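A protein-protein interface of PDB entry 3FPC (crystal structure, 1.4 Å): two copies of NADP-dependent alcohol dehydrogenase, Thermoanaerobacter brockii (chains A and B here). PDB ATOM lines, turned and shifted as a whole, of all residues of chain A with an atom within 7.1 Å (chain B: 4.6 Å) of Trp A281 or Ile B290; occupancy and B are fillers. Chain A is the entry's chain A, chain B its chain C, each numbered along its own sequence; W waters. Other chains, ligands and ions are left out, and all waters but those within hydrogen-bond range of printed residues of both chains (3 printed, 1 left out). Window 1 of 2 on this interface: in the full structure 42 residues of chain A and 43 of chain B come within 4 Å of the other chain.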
ATOM      1  N   VAL A 253      12.206   3.492 -22.177  1.00  0.00           N
ATOM      2  CA  VAL A 253      12.497   2.325 -21.349  1.00  0.00           C
ATOM      3  C   VAL A 253      11.364   1.318 -21.356  1.00  0.00           C
ATOM      4  O   VAL A 253      11.583   0.099 -21.388  1.00  0.00           O
ATOM      5  CB  VAL A 253      12.853   2.758 -19.909  1.00  0.00           C
ATOM      6  CG1 VAL A 253      12.883   1.578 -18.943  1.00  0.00           C
ATOM      7  CG2 VAL A 253      14.233   3.531 -19.935  1.00  0.00           C
ATOM      8  N   LYS A 254      10.130   1.819 -21.302  1.00  0.00           N
ATOM      9  CA  LYS A 254       8.960   0.945 -21.238  1.00  0.00           C
ATOM     10  C   LYS A 254       8.662   0.207 -22.538  1.00  0.00           C
ATOM     11  O   LYS A 254       8.009  -0.837 -22.488  1.00  0.00           O
ATOM     12  CB  LYS A 254       7.741   1.755 -20.820  1.00  0.00           C
ATOM     13  CG  LYS A 254       7.836   2.236 -19.368  1.00  0.00           C
ATOM     14  CD  LYS A 254       6.722   3.202 -18.969  1.00  0.00           C
ATOM     15  CE  LYS A 254       6.995   3.771 -17.580  1.00  0.00           C
ATOM     16  NZ  LYS A 254       5.949   4.783 -17.208  1.00  0.00           N
ATOM     17  N   ILE A 256      11.140  -0.743 -24.828  1.00  0.00           N
ATOM     18  CA  ILE A 256      12.348  -1.374 -25.347  1.00  0.00           C
ATOM     19  C   ILE A 256      12.597  -2.719 -24.649  1.00  0.00           C
ATOM     20  O   ILE A 256      12.240  -2.918 -23.472  1.00  0.00           O
ATOM     21  CB  ILE A 256      13.549  -0.428 -25.256  1.00  0.00           C
ATOM     22  CG1 ILE A 256      14.638  -0.770 -26.260  1.00  0.00           C
ATOM     23  CG2 ILE A 256      14.105  -0.368 -23.804  1.00  0.00           C
ATOM     24  CD1 ILE A 256      15.757   0.263 -26.308  1.00  0.00           C
ATOM     25  N   ILE A 262      19.149   2.986 -25.972  1.00  0.00           N
ATOM     26  CA  ILE A 262      18.391   4.211 -26.206  1.00  0.00           C
ATOM     27  C   ILE A 262      19.393   5.301 -26.527  1.00  0.00           C
ATOM     28  O   ILE A 262      20.264   5.609 -25.727  1.00  0.00           O
ATOM     29  CB  ILE A 262      17.556   4.598 -24.959  1.00  0.00           C
ATOM     30  CG1 ILE A 262      16.541   3.490 -24.612  1.00  0.00           C
ATOM     31  CG2 ILE A 262      16.899   5.965 -25.147  1.00  0.00           C
ATOM     32  CD1 ILE A 262      15.982   3.571 -23.126  1.00  0.00           C
ATOM     33  N   ILE A 276      14.195   7.827 -14.812  1.00  0.00           N
ATOM     34  CA  ILE A 276      14.240   6.459 -15.375  1.00  0.00           C
ATOM     35  C   ILE A 276      13.452   5.560 -14.415  1.00  0.00           C
ATOM     36  O   ILE A 276      13.789   5.488 -13.234  1.00  0.00           O
ATOM     37  CB  ILE A 276      15.682   5.952 -15.513  1.00  0.00           C
ATOM     38  CG1 ILE A 276      16.513   6.937 -16.354  1.00  0.00           C
ATOM     39  CG2 ILE A 276      15.748   4.544 -16.071  1.00  0.00           C
ATOM     40  CD1 ILE A 276      15.976   7.206 -17.790  1.00  0.00           C
ATOM     41  N   PRO A 277      12.408   4.883 -14.916  1.00  0.00           N
ATOM     42  CA  PRO A 277      11.557   4.102 -14.021  1.00  0.00           C
ATOM     43  C   PRO A 277      12.280   2.856 -13.501  1.00  0.00           C
ATOM     44  O   PRO A 277      12.754   2.035 -14.275  1.00  0.00           O
ATOM     45  CB  PRO A 277      10.358   3.734 -14.909  1.00  0.00           C
ATOM     46  CG  PRO A 277      10.901   3.739 -16.276  1.00  0.00           C
ATOM     47  CD  PRO A 277      11.915   4.836 -16.308  1.00  0.00           C
ATOM     48  N   ARG A 278      12.318   2.696 -12.180  1.00  0.00           N
ATOM     49  CA  ARG A 278      13.114   1.643 -11.566  1.00  0.00           C
ATOM     50  C   ARG A 278      12.696   0.263 -12.003  1.00  0.00           C
ATOM     51  O   ARG A 278      13.550  -0.512 -12.437  1.00  0.00           O
ATOM     52  CB  ARG A 278      13.036   1.744 -10.058  1.00  0.00           C
ATOM     53  CG  ARG A 278      13.871   0.687  -9.304  1.00  0.00           C
ATOM     54  CD  ARG A 278      13.753   0.772  -7.776  1.00  0.00           C
ATOM     55  NE  ARG A 278      12.377   0.497  -7.363  1.00  0.00           N
ATOM     56  CZ  ARG A 278      11.870  -0.694  -7.058  1.00  0.00           C
ATOM     57  NH1 ARG A 278      12.613  -1.780  -6.965  1.00  0.00           N
ATOM     58  NH2 ARG A 278      10.576  -0.799  -6.826  1.00  0.00           N
ATOM     59  N   SER A 279      11.416  -0.070 -11.911  1.00  0.00           N
ATOM     60  CA  SER A 279      10.977  -1.438 -12.242  1.00  0.00           C
ATOM     61  C   SER A 279      11.213  -1.780 -13.717  1.00  0.00           C
ATOM     62  O   SER A 279      11.781  -2.829 -14.026  1.00  0.00           O
ATOM     63  CB  SER A 279       9.515  -1.626 -11.868  1.00  0.00           C
ATOM     64  OG  SER A 279       9.355  -1.578 -10.452  1.00  0.00           O
ATOM     65  N   GLU A 280      10.830  -0.880 -14.619  1.00  0.00           N
ATOM     66  CA  GLU A 280      10.959  -1.149 -16.055  1.00  0.00           C
ATOM     67  C   GLU A 280      12.396  -1.072 -16.558  1.00  0.00           C
ATOM     68  O   GLU A 280      12.686  -1.591 -17.630  1.00  0.00           O
ATOM     69  CB  GLU A 280      10.052  -0.255 -16.887  1.00  0.00           C
ATOM     70  CG  GLU A 280       8.542  -0.516 -16.592  1.00  0.00           C
ATOM     71  CD  GLU A 280       7.941   0.289 -15.500  1.00  0.00           C
ATOM     72  OE1 GLU A 280       8.647   0.817 -14.618  1.00  0.00           O
ATOM     73  OE2 GLU A 280       6.680   0.428 -15.532  1.00  0.00           O
ATOM     74  N   TRP A 281      13.288  -0.468 -15.765  1.00  0.00           N
ATOM     75  CA  TRP A 281      14.709  -0.522 -16.027  1.00  0.00           C
ATOM     76  C   TRP A 281      15.340  -1.740 -15.393  1.00  0.00           C
ATOM     77  O   TRP A 281      16.573  -1.823 -15.229  1.00  0.00           O
ATOM     78  CB  TRP A 281      15.373   0.762 -15.548  1.00  0.00           C
ATOM     79  CG  TRP A 281      16.636   1.109 -16.285  1.00  0.00           C
ATOM     80  CD1 TRP A 281      16.771   1.287 -17.617  1.00  0.00           C
ATOM     81  CD2 TRP A 281      17.942   1.384 -15.719  1.00  0.00           C
ATOM     82  NE1 TRP A 281      18.054   1.641 -17.924  1.00  0.00           N
ATOM     83  CE2 TRP A 281      18.801   1.677 -16.780  1.00  0.00           C
ATOM     84  CE3 TRP A 281      18.463   1.332 -14.431  1.00  0.00           C
ATOM     85  CZ2 TRP A 281      20.173   1.913 -16.601  1.00  0.00           C
ATOM     86  CZ3 TRP A 281      19.810   1.585 -14.253  1.00  0.00           C
ATOM     87  CH2 TRP A 281      20.645   1.856 -15.340  1.00  0.00           C
ATOM     88  N   GLY A 282      14.520  -2.707 -15.027  1.00  0.00           N
ATOM     89  CA  GLY A 282      15.058  -3.979 -14.505  1.00  0.00           C
ATOM     90  C   GLY A 282      15.658  -3.835 -13.133  1.00  0.00           C
ATOM     91  O   GLY A 282      16.596  -4.547 -12.792  1.00  0.00           O
ATOM     92  N   VAL A 283      15.080  -2.940 -12.342  1.00  0.00           N
ATOM     93  CA  VAL A 283      15.568  -2.636 -10.984  1.00  0.00           C
ATOM     94  C   VAL A 283      17.097  -2.435 -10.970  1.00  0.00           C
ATOM     95  O   VAL A 283      17.781  -2.762 -10.002  1.00  0.00           O
ATOM     96  CB  VAL A 283      15.002  -3.586  -9.868  1.00  0.00           C
ATOM     97  CG1 VAL A 283      13.481  -3.479  -9.790  1.00  0.00           C
ATOM     98  CG2 VAL A 283      15.431  -5.024 -10.062  1.00  0.00           C
ATOM     99  N   GLY A 284      17.591  -1.775 -12.027  1.00  0.00           N
ATOM    100  CA  GLY A 284      19.002  -1.448 -12.174  1.00  0.00           C
ATOM    101  C   GLY A 284      19.793  -2.384 -13.085  1.00  0.00           C
ATOM    102  O   GLY A 284      20.985  -2.166 -13.299  1.00  0.00           O
ATOM    103  N   MET A 285      19.149  -3.463 -13.545  1.00  0.00           N
ATOM    104  CA  MET A 285      19.867  -4.619 -14.071  1.00  0.00           C
ATOM    105  C   MET A 285      19.342  -5.140 -15.430  1.00  0.00           C
ATOM    106  O   MET A 285      19.696  -6.237 -15.848  1.00  0.00           O
ATOM    107  CB  MET A 285      19.824  -5.727 -13.044  1.00  0.00           C
ATOM    108  CG  MET A 285      20.466  -5.362 -11.709  1.00  0.00           C
ATOM    109  SD  MET A 285      20.503  -6.693 -10.510  1.00  0.00           S
ATOM    110  CE  MET A 285      18.719  -6.899 -10.137  1.00  0.00           C
ATOM    111  N   GLY A 286      18.558  -4.330 -16.133  1.00  0.00           N
ATOM    112  CA  GLY A 286      17.910  -4.801 -17.387  1.00  0.00           C
ATOM    113  C   GLY A 286      18.724  -4.640 -18.656  1.00  0.00           C
ATOM    114  O   GLY A 286      18.207  -4.923 -19.722  1.00  0.00           O
ATOM    115  N   HIS A 287      19.968  -4.157 -18.564  1.00  0.00           N
ATOM    116  CA  HIS A 287      20.806  -3.873 -19.704  1.00  0.00           C
ATOM    117  C   HIS A 287      20.090  -2.997 -20.759  1.00  0.00           C
ATOM    118  O   HIS A 287      20.279  -3.187 -21.957  1.00  0.00           O
ATOM    119  CB  HIS A 287      21.410  -5.115 -20.368  1.00  0.00           C
ATOM    120  CG  HIS A 287      22.380  -5.878 -19.531  1.00  0.00           C
ATOM    121  ND1 HIS A 287      22.008  -6.937 -18.737  1.00  0.00           N
ATOM    122  CD2 HIS A 287      23.726  -5.750 -19.394  1.00  0.00           C
ATOM    123  CE1 HIS A 287      23.089  -7.426 -18.147  1.00  0.00           C
ATOM    124  NE2 HIS A 287      24.145  -6.729 -18.530  1.00  0.00           N
ATOM    125  N   LYS A 288      19.333  -2.013 -20.285  1.00  0.00           N
ATOM    126  CA  LYS A 288      18.749  -1.003 -21.148  1.00  0.00           C
ATOM    127  C   LYS A 288      19.685   0.219 -21.126  1.00  0.00           C
ATOM    128  O   LYS A 288      19.582   1.092 -20.274  1.00  0.00           O
ATOM    129  CB  LYS A 288      17.310  -0.660 -20.722  1.00  0.00           C
ATOM    130  CG  LYS A 288      16.346  -1.834 -20.886  1.00  0.00           C
ATOM    131  CD  LYS A 288      14.951  -1.533 -20.443  1.00  0.00           C
ATOM    132  CE  LYS A 288      13.971  -2.689 -20.691  1.00  0.00           C
ATOM    133  NZ  LYS A 288      12.569  -2.373 -20.341  1.00  0.00           N
ATOM    134  N   HIS A 289      20.653   0.208 -22.029  1.00  0.00           N
ATOM    135  CA  HIS A 289      21.744   1.190 -22.012  1.00  0.00           C
ATOM    136  C   HIS A 289      21.192   2.529 -22.478  1.00  0.00           C
ATOM    137  O   HIS A 289      20.417   2.580 -23.442  1.00  0.00           O
ATOM    138  CB  HIS A 289      22.845   0.752 -22.970  1.00  0.00           C
ATOM    139  CG  HIS A 289      23.396  -0.606 -22.674  1.00  0.00           C
ATOM    140  ND1 HIS A 289      24.203  -0.853 -21.607  1.00  0.00           N
ATOM    141  CD2 HIS A 289      23.259  -1.786 -23.325  1.00  0.00           C
ATOM    142  CE1 HIS A 289      24.525  -2.137 -21.585  1.00  0.00           C
ATOM    143  NE2 HIS A 289      23.970  -2.724 -22.624  1.00  0.00           N
ATOM    144  N   ILE A 290      21.603   3.598 -21.810  1.00  0.00           N
ATOM    145  CA  ILE A 290      21.099   4.945 -22.064  1.00  0.00           C
ATOM    146  C   ILE A 290      22.252   5.834 -22.508  1.00  0.00           C
ATOM    147  O   ILE A 290      23.275   5.969 -21.816  1.00  0.00           O
ATOM    148  CB  ILE A 290      20.384   5.532 -20.846  1.00  0.00           C
ATOM    149  CG1 ILE A 290      19.163   4.683 -20.426  1.00  0.00           C
ATOM    150  CG2 ILE A 290      19.948   6.959 -21.128  1.00  0.00           C
ATOM    151  CD1 ILE A 290      18.633   5.079 -19.019  1.00  0.00           C
ATOM    152  N   HIS A 291      22.066   6.442 -23.669  1.00  0.00           N
ATOM    153  CA  HIS A 291      23.084   7.266 -24.270  1.00  0.00           C
ATOM    154  C   HIS A 291      22.462   8.627 -24.611  1.00  0.00           C
ATOM    155  O   HIS A 291      21.271   8.721 -24.946  1.00  0.00           O
ATOM    156  CB  HIS A 291      23.615   6.613 -25.539  1.00  0.00           C
ATOM    157  CG  HIS A 291      23.888   5.155 -25.460  1.00  0.00           C
ATOM    158  ND1 HIS A 291      25.053   4.660 -24.920  1.00  0.00           N
ATOM    159  CD2 HIS A 291      23.170   4.079 -25.868  1.00  0.00           C
ATOM    160  CE1 HIS A 291      25.036   3.334 -24.986  1.00  0.00           C
ATOM    161  NE2 HIS A 291      23.907   2.951 -25.559  1.00  0.00           N
ATOM    162  N   GLY A 292      23.257   9.662 -24.506  1.00  0.00           N
ATOM    163  CA  GLY A 292      22.810  10.972 -24.925  1.00  0.00           C
ATOM    164  C   GLY A 292      23.995  11.838 -25.282  1.00  0.00           C
ATOM    165  O   GLY A 292      24.862  12.095 -24.438  1.00  0.00           O
ATOM    166  N   MET B 106      13.089 -10.117 -18.959  1.00  0.00           N
ATOM    167  CA  MET B 106      13.996  -9.301 -18.180  1.00  0.00           C
ATOM    168  C   MET B 106      14.242  -9.963 -16.839  1.00  0.00           C
ATOM    169  O   MET B 106      13.301 -10.322 -16.102  1.00  0.00           O
ATOM    170  CB  MET B 106      13.443  -7.877 -18.013  1.00  0.00           C
ATOM    171  CG  MET B 106      14.436  -6.909 -17.399  1.00  0.00           C
ATOM    172  SD  MET B 106      14.085  -5.175 -17.742  1.00  0.00           S
ATOM    173  CE  MET B 106      12.429  -5.041 -17.064  1.00  0.00           C
ATOM    174  N   PHE B 249      22.953   7.552  -8.813  1.00  0.00           N
ATOM    175  CA  PHE B 249      23.241   7.846 -10.201  1.00  0.00           C
ATOM    176  C   PHE B 249      23.548   9.312 -10.412  1.00  0.00           C
ATOM    177  O   PHE B 249      24.442   9.669 -11.192  1.00  0.00           O
ATOM    178  CB  PHE B 249      22.102   7.409 -11.105  1.00  0.00           C
ATOM    179  CG  PHE B 249      22.011   5.904 -11.241  1.00  0.00           C
ATOM    180  CD1 PHE B 249      21.504   5.133 -10.203  1.00  0.00           C
ATOM    181  CD2 PHE B 249      22.456   5.265 -12.363  1.00  0.00           C
ATOM    182  CE1 PHE B 249      21.447   3.760 -10.327  1.00  0.00           C
ATOM    183  CE2 PHE B 249      22.404   3.876 -12.490  1.00  0.00           C
ATOM    184  CZ  PHE B 249      21.868   3.133 -11.483  1.00  0.00           C
ATOM    185  N   ILE B 262      29.113   4.929 -16.907  1.00  0.00           N
ATOM    186  CA  ILE B 262      28.674   4.535 -15.560  1.00  0.00           C
ATOM    187  C   ILE B 262      28.112   3.139 -15.635  1.00  0.00           C
ATOM    188  O   ILE B 262      27.146   2.903 -16.364  1.00  0.00           O
ATOM    189  CB  ILE B 262      27.579   5.513 -15.008  1.00  0.00           C
ATOM    190  CG1 ILE B 262      28.145   6.915 -14.887  1.00  0.00           C
ATOM    191  CG2 ILE B 262      27.032   5.042 -13.672  1.00  0.00           C
ATOM    192  CD1 ILE B 262      27.033   8.025 -14.820  1.00  0.00           C
ATOM    193  N   ASN B 264      26.360   0.330 -13.619  1.00  0.00           N
ATOM    194  CA  ASN B 264      25.648  -0.077 -12.426  1.00  0.00           C
ATOM    195  C   ASN B 264      25.438  -1.592 -12.367  1.00  0.00           C
ATOM    196  O   ASN B 264      24.953  -2.196 -13.319  1.00  0.00           O
ATOM    197  CB  ASN B 264      24.287   0.571 -12.323  1.00  0.00           C
ATOM    198  CG  ASN B 264      23.553   0.093 -11.095  1.00  0.00           C
ATOM    199  OD1 ASN B 264      24.006   0.344  -9.969  1.00  0.00           O
ATOM    200  ND2 ASN B 264      22.423  -0.647 -11.286  1.00  0.00           N
ATOM    201  N   ILE B 274      14.894   6.631 -10.947  1.00  0.00           N
ATOM    202  CA  ILE B 274      16.284   7.013 -10.893  1.00  0.00           C
ATOM    203  C   ILE B 274      16.389   8.372 -11.581  1.00  0.00           C
ATOM    204  O   ILE B 274      16.017   8.491 -12.745  1.00  0.00           O
ATOM    205  CB  ILE B 274      17.154   6.002 -11.657  1.00  0.00           C
ATOM    206  CG1 ILE B 274      17.049   4.605 -11.040  1.00  0.00           C
ATOM    207  CG2 ILE B 274      18.629   6.528 -11.695  1.00  0.00           C
ATOM    208  CD1 ILE B 274      17.365   3.496 -12.061  1.00  0.00           C
ATOM    209  N   ILE B 276      18.319  11.427 -13.173  1.00  0.00           N
ATOM    210  CA  ILE B 276      19.566  11.832 -13.829  1.00  0.00           C
ATOM    211  C   ILE B 276      19.495  13.362 -13.946  1.00  0.00           C
ATOM    212  O   ILE B 276      18.584  13.901 -14.575  1.00  0.00           O
ATOM    213  CB  ILE B 276      19.691  11.184 -15.206  1.00  0.00           C
ATOM    214  CG1 ILE B 276      19.670   9.681 -15.071  1.00  0.00           C
ATOM    215  CG2 ILE B 276      20.946  11.657 -15.944  1.00  0.00           C
ATOM    216  CD1 ILE B 276      20.769   9.078 -14.141  1.00  0.00           C
ATOM    217  N   TRP B 281      24.193  16.180 -16.872  1.00  0.00           N
ATOM    218  CA  TRP B 281      24.183  15.198 -17.988  1.00  0.00           C
ATOM    219  C   TRP B 281      24.349  15.888 -19.353  1.00  0.00           C
ATOM    220  O   TRP B 281      24.082  15.279 -20.410  1.00  0.00           O
ATOM    221  CB  TRP B 281      22.893  14.330 -17.915  1.00  0.00           C
ATOM    222  CG  TRP B 281      23.037  12.975 -18.500  1.00  0.00           C
ATOM    223  CD1 TRP B 281      23.979  12.043 -18.172  1.00  0.00           C
ATOM    224  CD2 TRP B 281      22.240  12.380 -19.545  1.00  0.00           C
ATOM    225  NE1 TRP B 281      23.786  10.896 -18.898  1.00  0.00           N
ATOM    226  CE2 TRP B 281      22.750  11.097 -19.777  1.00  0.00           C
ATOM    227  CE3 TRP B 281      21.162  12.817 -20.313  1.00  0.00           C
ATOM    228  CZ2 TRP B 281      22.220  10.244 -20.762  1.00  0.00           C
ATOM    229  CZ3 TRP B 281      20.650  11.987 -21.286  1.00  0.00           C
ATOM    230  CH2 TRP B 281      21.170  10.701 -21.494  1.00  0.00           C
ATOM    231  N   LYS B 288      27.592  10.875 -21.357  1.00  0.00           N
ATOM    232  CA  LYS B 288      27.767  10.155 -20.101  1.00  0.00           C
ATOM    233  C   LYS B 288      26.877   8.940 -20.141  1.00  0.00           C
ATOM    234  O   LYS B 288      25.695   8.999 -19.820  1.00  0.00           O
ATOM    235  CB  LYS B 288      27.490  11.078 -18.896  1.00  0.00           C
ATOM    236  CG  LYS B 288      28.452  12.277 -18.802  1.00  0.00           C
ATOM    237  CD  LYS B 288      28.182  13.136 -17.591  1.00  0.00           C
ATOM    238  CE  LYS B 288      29.218  14.218 -17.436  1.00  0.00           C
ATOM    239  NZ  LYS B 288      28.991  15.054 -16.202  1.00  0.00           N
ATOM    240  N   HIS B 289      27.422   7.860 -20.685  1.00  0.00           N
ATOM    241  CA  HIS B 289      26.659   6.631 -20.961  1.00  0.00           C
ATOM    242  C   HIS B 289      26.310   5.915 -19.677  1.00  0.00           C
ATOM    243  O   HIS B 289      27.163   5.833 -18.798  1.00  0.00           O
ATOM    244  CB  HIS B 289      27.451   5.716 -21.884  1.00  0.00           C
ATOM    245  CG  HIS B 289      27.916   6.359 -23.141  1.00  0.00           C
ATOM    246  ND1 HIS B 289      27.071   6.648 -24.172  1.00  0.00           N
ATOM    247  CD2 HIS B 289      29.146   6.712 -23.561  1.00  0.00           C
ATOM    248  CE1 HIS B 289      27.751   7.216 -25.159  1.00  0.00           C
ATOM    249  NE2 HIS B 289      29.019   7.259 -24.811  1.00  0.00           N
ATOM    250  N   ILE B 290      25.052   5.450 -19.564  1.00  0.00           N
ATOM    251  CA  ILE B 290      24.546   4.823 -18.333  1.00  0.00           C
ATOM    252  C   ILE B 290      24.156   3.389 -18.630  1.00  0.00           C
ATOM    253  O   ILE B 290      23.365   3.112 -19.532  1.00  0.00           O
ATOM    254  CB  ILE B 290      23.351   5.593 -17.744  1.00  0.00           C
ATOM    255  CG1 ILE B 290      23.775   7.026 -17.420  1.00  0.00           C
ATOM    256  CG2 ILE B 290      22.823   4.882 -16.458  1.00  0.00           C
ATOM    257  CD1 ILE B 290      22.621   7.926 -17.090  1.00  0.00           C
ATOM    258  N   HIS B 291      24.730   2.480 -17.865  1.00  0.00           N
ATOM    259  CA  HIS B 291      24.525   1.071 -18.041  1.00  0.00           C
ATOM    260  C   HIS B 291      24.090   0.495 -16.688  1.00  0.00           C
ATOM    261  O   HIS B 291      24.470   0.978 -15.616  1.00  0.00           O
ATOM    262  CB  HIS B 291      25.816   0.390 -18.483  1.00  0.00           C
ATOM    263  CG  HIS B 291      26.563   1.069 -19.569  1.00  0.00           C
ATOM    264  ND1 HIS B 291      26.231   0.935 -20.897  1.00  0.00           N
ATOM    265  CD2 HIS B 291      27.613   1.925 -19.511  1.00  0.00           C
ATOM    266  CE1 HIS B 291      27.065   1.686 -21.618  1.00  0.00           C
ATOM    267  NE2 HIS B 291      27.917   2.286 -20.796  1.00  0.00           N
ATOM    268  N   GLY B 292      23.257  -0.514 -16.731  1.00  0.00           N
ATOM    269  CA  GLY B 292      22.850  -1.217 -15.516  1.00  0.00           C
ATOM    270  C   GLY B 292      22.434  -2.628 -15.870  1.00  0.00           C
ATOM    271  O   GLY B 292      21.484  -2.814 -16.636  1.00  0.00           O
HETATM  272  O   HOH W   1      25.622   9.117 -23.125  1.00  0.00           O
HETATM  273  O   HOH W   2      22.101  -0.765 -19.299  1.00  0.00           O
HETATM  274  O   HOH W   3      25.066  12.541 -21.540  1.00  0.00           O
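The backbone carbonyl oxygen (O) of Ile A276 is in hydrogen-bond range of the backbone NH (N) of Ile B274. The backbone NH of Gly A282 sits close to the side-chain sulfur of Met B106, 3.7 Å away. The backbone carbonyl oxygen (O) of Gly A284 is in hydrogen-bond range of the side-chain amide nitrogen (ND2) of Asn B264 (2.9 Å). The backbone NH (N) of Gly A286 lies within hydrogen-bond range of the backbone carbonyl oxygen (O) of Gly B292 (3.3 Å). The backbone carbonyl oxygen of Gly B292 sits at hydrogen-bond distance from the backbone NH of His A287 (2.8 Å). ND1 of His A289 is in hydrogen-bond range of ND1 of His B291, at 2.8 Å. The backbone NH of Ile B290 lies within hydrogen-bond range of the backbone carbonyl oxygen of Ile A290 (2.9 Å). A ring nitrogen (ND1) of His B289 is in hydrogen-bond range of a ring nitrogen (ND1) of His A291 (2.9 Å). The backbone carbonyl oxygen (O) of Gly B292 sits close to the backbone carbonyl oxygen (O) of Gly A284 (3.4 Å).
The backbone carbonyl oxygen (O) of Val A253 lies within hydrogen-bond range of the side-chain amino group (NZ) of Lys A288, 2.9 Å away. The backbone carbonyl oxygen (O) of Trp A281 sits at hydrogen-bond distance from the backbone NH (N) of Gly A286, at 3.3 Å. NE1 of Trp A281 lies within hydrogen-bond range of O of Lys A288. N of Ile B262 is in hydrogen-bond range of O of His B289 (2.9 Å). The backbone NH (N) of His B291 is in hydrogen-bond range of the backbone carbonyl oxygen (O) of Ile B262, 2.9 Å away. N of Asn B264 sits at hydrogen-bond distance from O of His B291, at 2.8 Å.
Among the printed residues, merely in contact across the chains: Met A285 with Gly B292 (3.4 Å), Trp A281 with Ile B274 (3.4 Å), Glu A280 with Met B106 (3.5 Å), His A289 with Ile B290 (3.5 Å), Ile A290 with His B289 (3.6 Å), Trp A281 with Phe B249 (3.8 Å), Trp A281 with Gly B292 (3.8 Å), Gly A292 with Trp B281 (3.8 Å), Ser A279 with Met B106 (3.8 Å), Lys A288 with Met B106 (3.9 Å), Gly A286 with Met B106 (3.9 Å), Trp A281 with Ile B290 (3.9 Å), Trp A281 with His B291 (3.9 Å), Ile A290 with Trp B281 (3.95 Å) and His A291 with Trp B281 (3.96 Å).
Trp A281 touches just these residues of chain B: Phe B249 (3.8 Å), Ile B274 (3.4 Å), Ile B290 (3.9 Å), His B291 (3.9 Å) and Gly B292 (3.8 Å). Of chain A, only Trp A281, His A289 and Ile A290 come within 4 Å of Ile B290. Printed residues of chain B within 4 Å of Gly A286: Met B106 (3.9 Å) and Gly B292 (3.3 Å). Printed residues of chain A within 4 Å of Asn B264: Gly A284. Of the printed residues of chain A, His B289 touches Ile A290 and His A291. Printed residues of chain B within 4 Å of Glu A280: Met B106. Of the printed residues of chain A, Ile B274 touches Ile A276 (2.8 Å) and Trp A281 (3.4 Å). Ile B276 touches none of the printed residues of chain A. Ile B262 touches none of the printed residues of chain A. The nearest residue of chain B that does not touch Trp A281 is Met B106 (4.3 Å). The nearest printed residue of chain B that does not touch Glu A280 is Ile B274 (8.1 Å).
Of the 21 printed residues of chain A, 14 touch a printed residue of chain B. Hydrophobic or aromatic side chains of chain B that line the printed part of chain A: Met B106, Phe B249, Ile B274, Trp B281, His B289, Ile B290 and His B291.
Trp A281 touches Ile B290, and with the chains exchanged Ile A290 touches Trp B281. Trp A281 touches His B291, and with the chains exchanged His A291 touches Trp B281. Trp A281 touches Gly B292, and with the chains exchanged Gly A292 touches Trp B281. His A289 touches Ile B290, and with the chains exchanged Ile A290 touches His B289. Positions printed for both chains: 262, 276, 281, 288, 289, 290, 291 and 292.
Water W1 lies within hydrogen-bond range of the backbone NH (N) of Gly A292 (2.8 Å), a ring nitrogen (ND1) of His B289 (3.0 Å) and the backbone NH (N) of Lys B288 (3.2 Å). Water W2 lies within hydrogen-bond range of N of Gly B292 (2.8 Å), ND1 of His A289 (3.1 Å) and N of Lys A288 (3.2 Å). Water W3 lies within hydrogen-bond range of the backbone carbonyl oxygen (O) of Gly A292 (2.9 Å), the backbone NH (N) of Lys B288 (3.0 Å) and the backbone carbonyl oxygen (O) of Trp B281 (3.1 Å).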
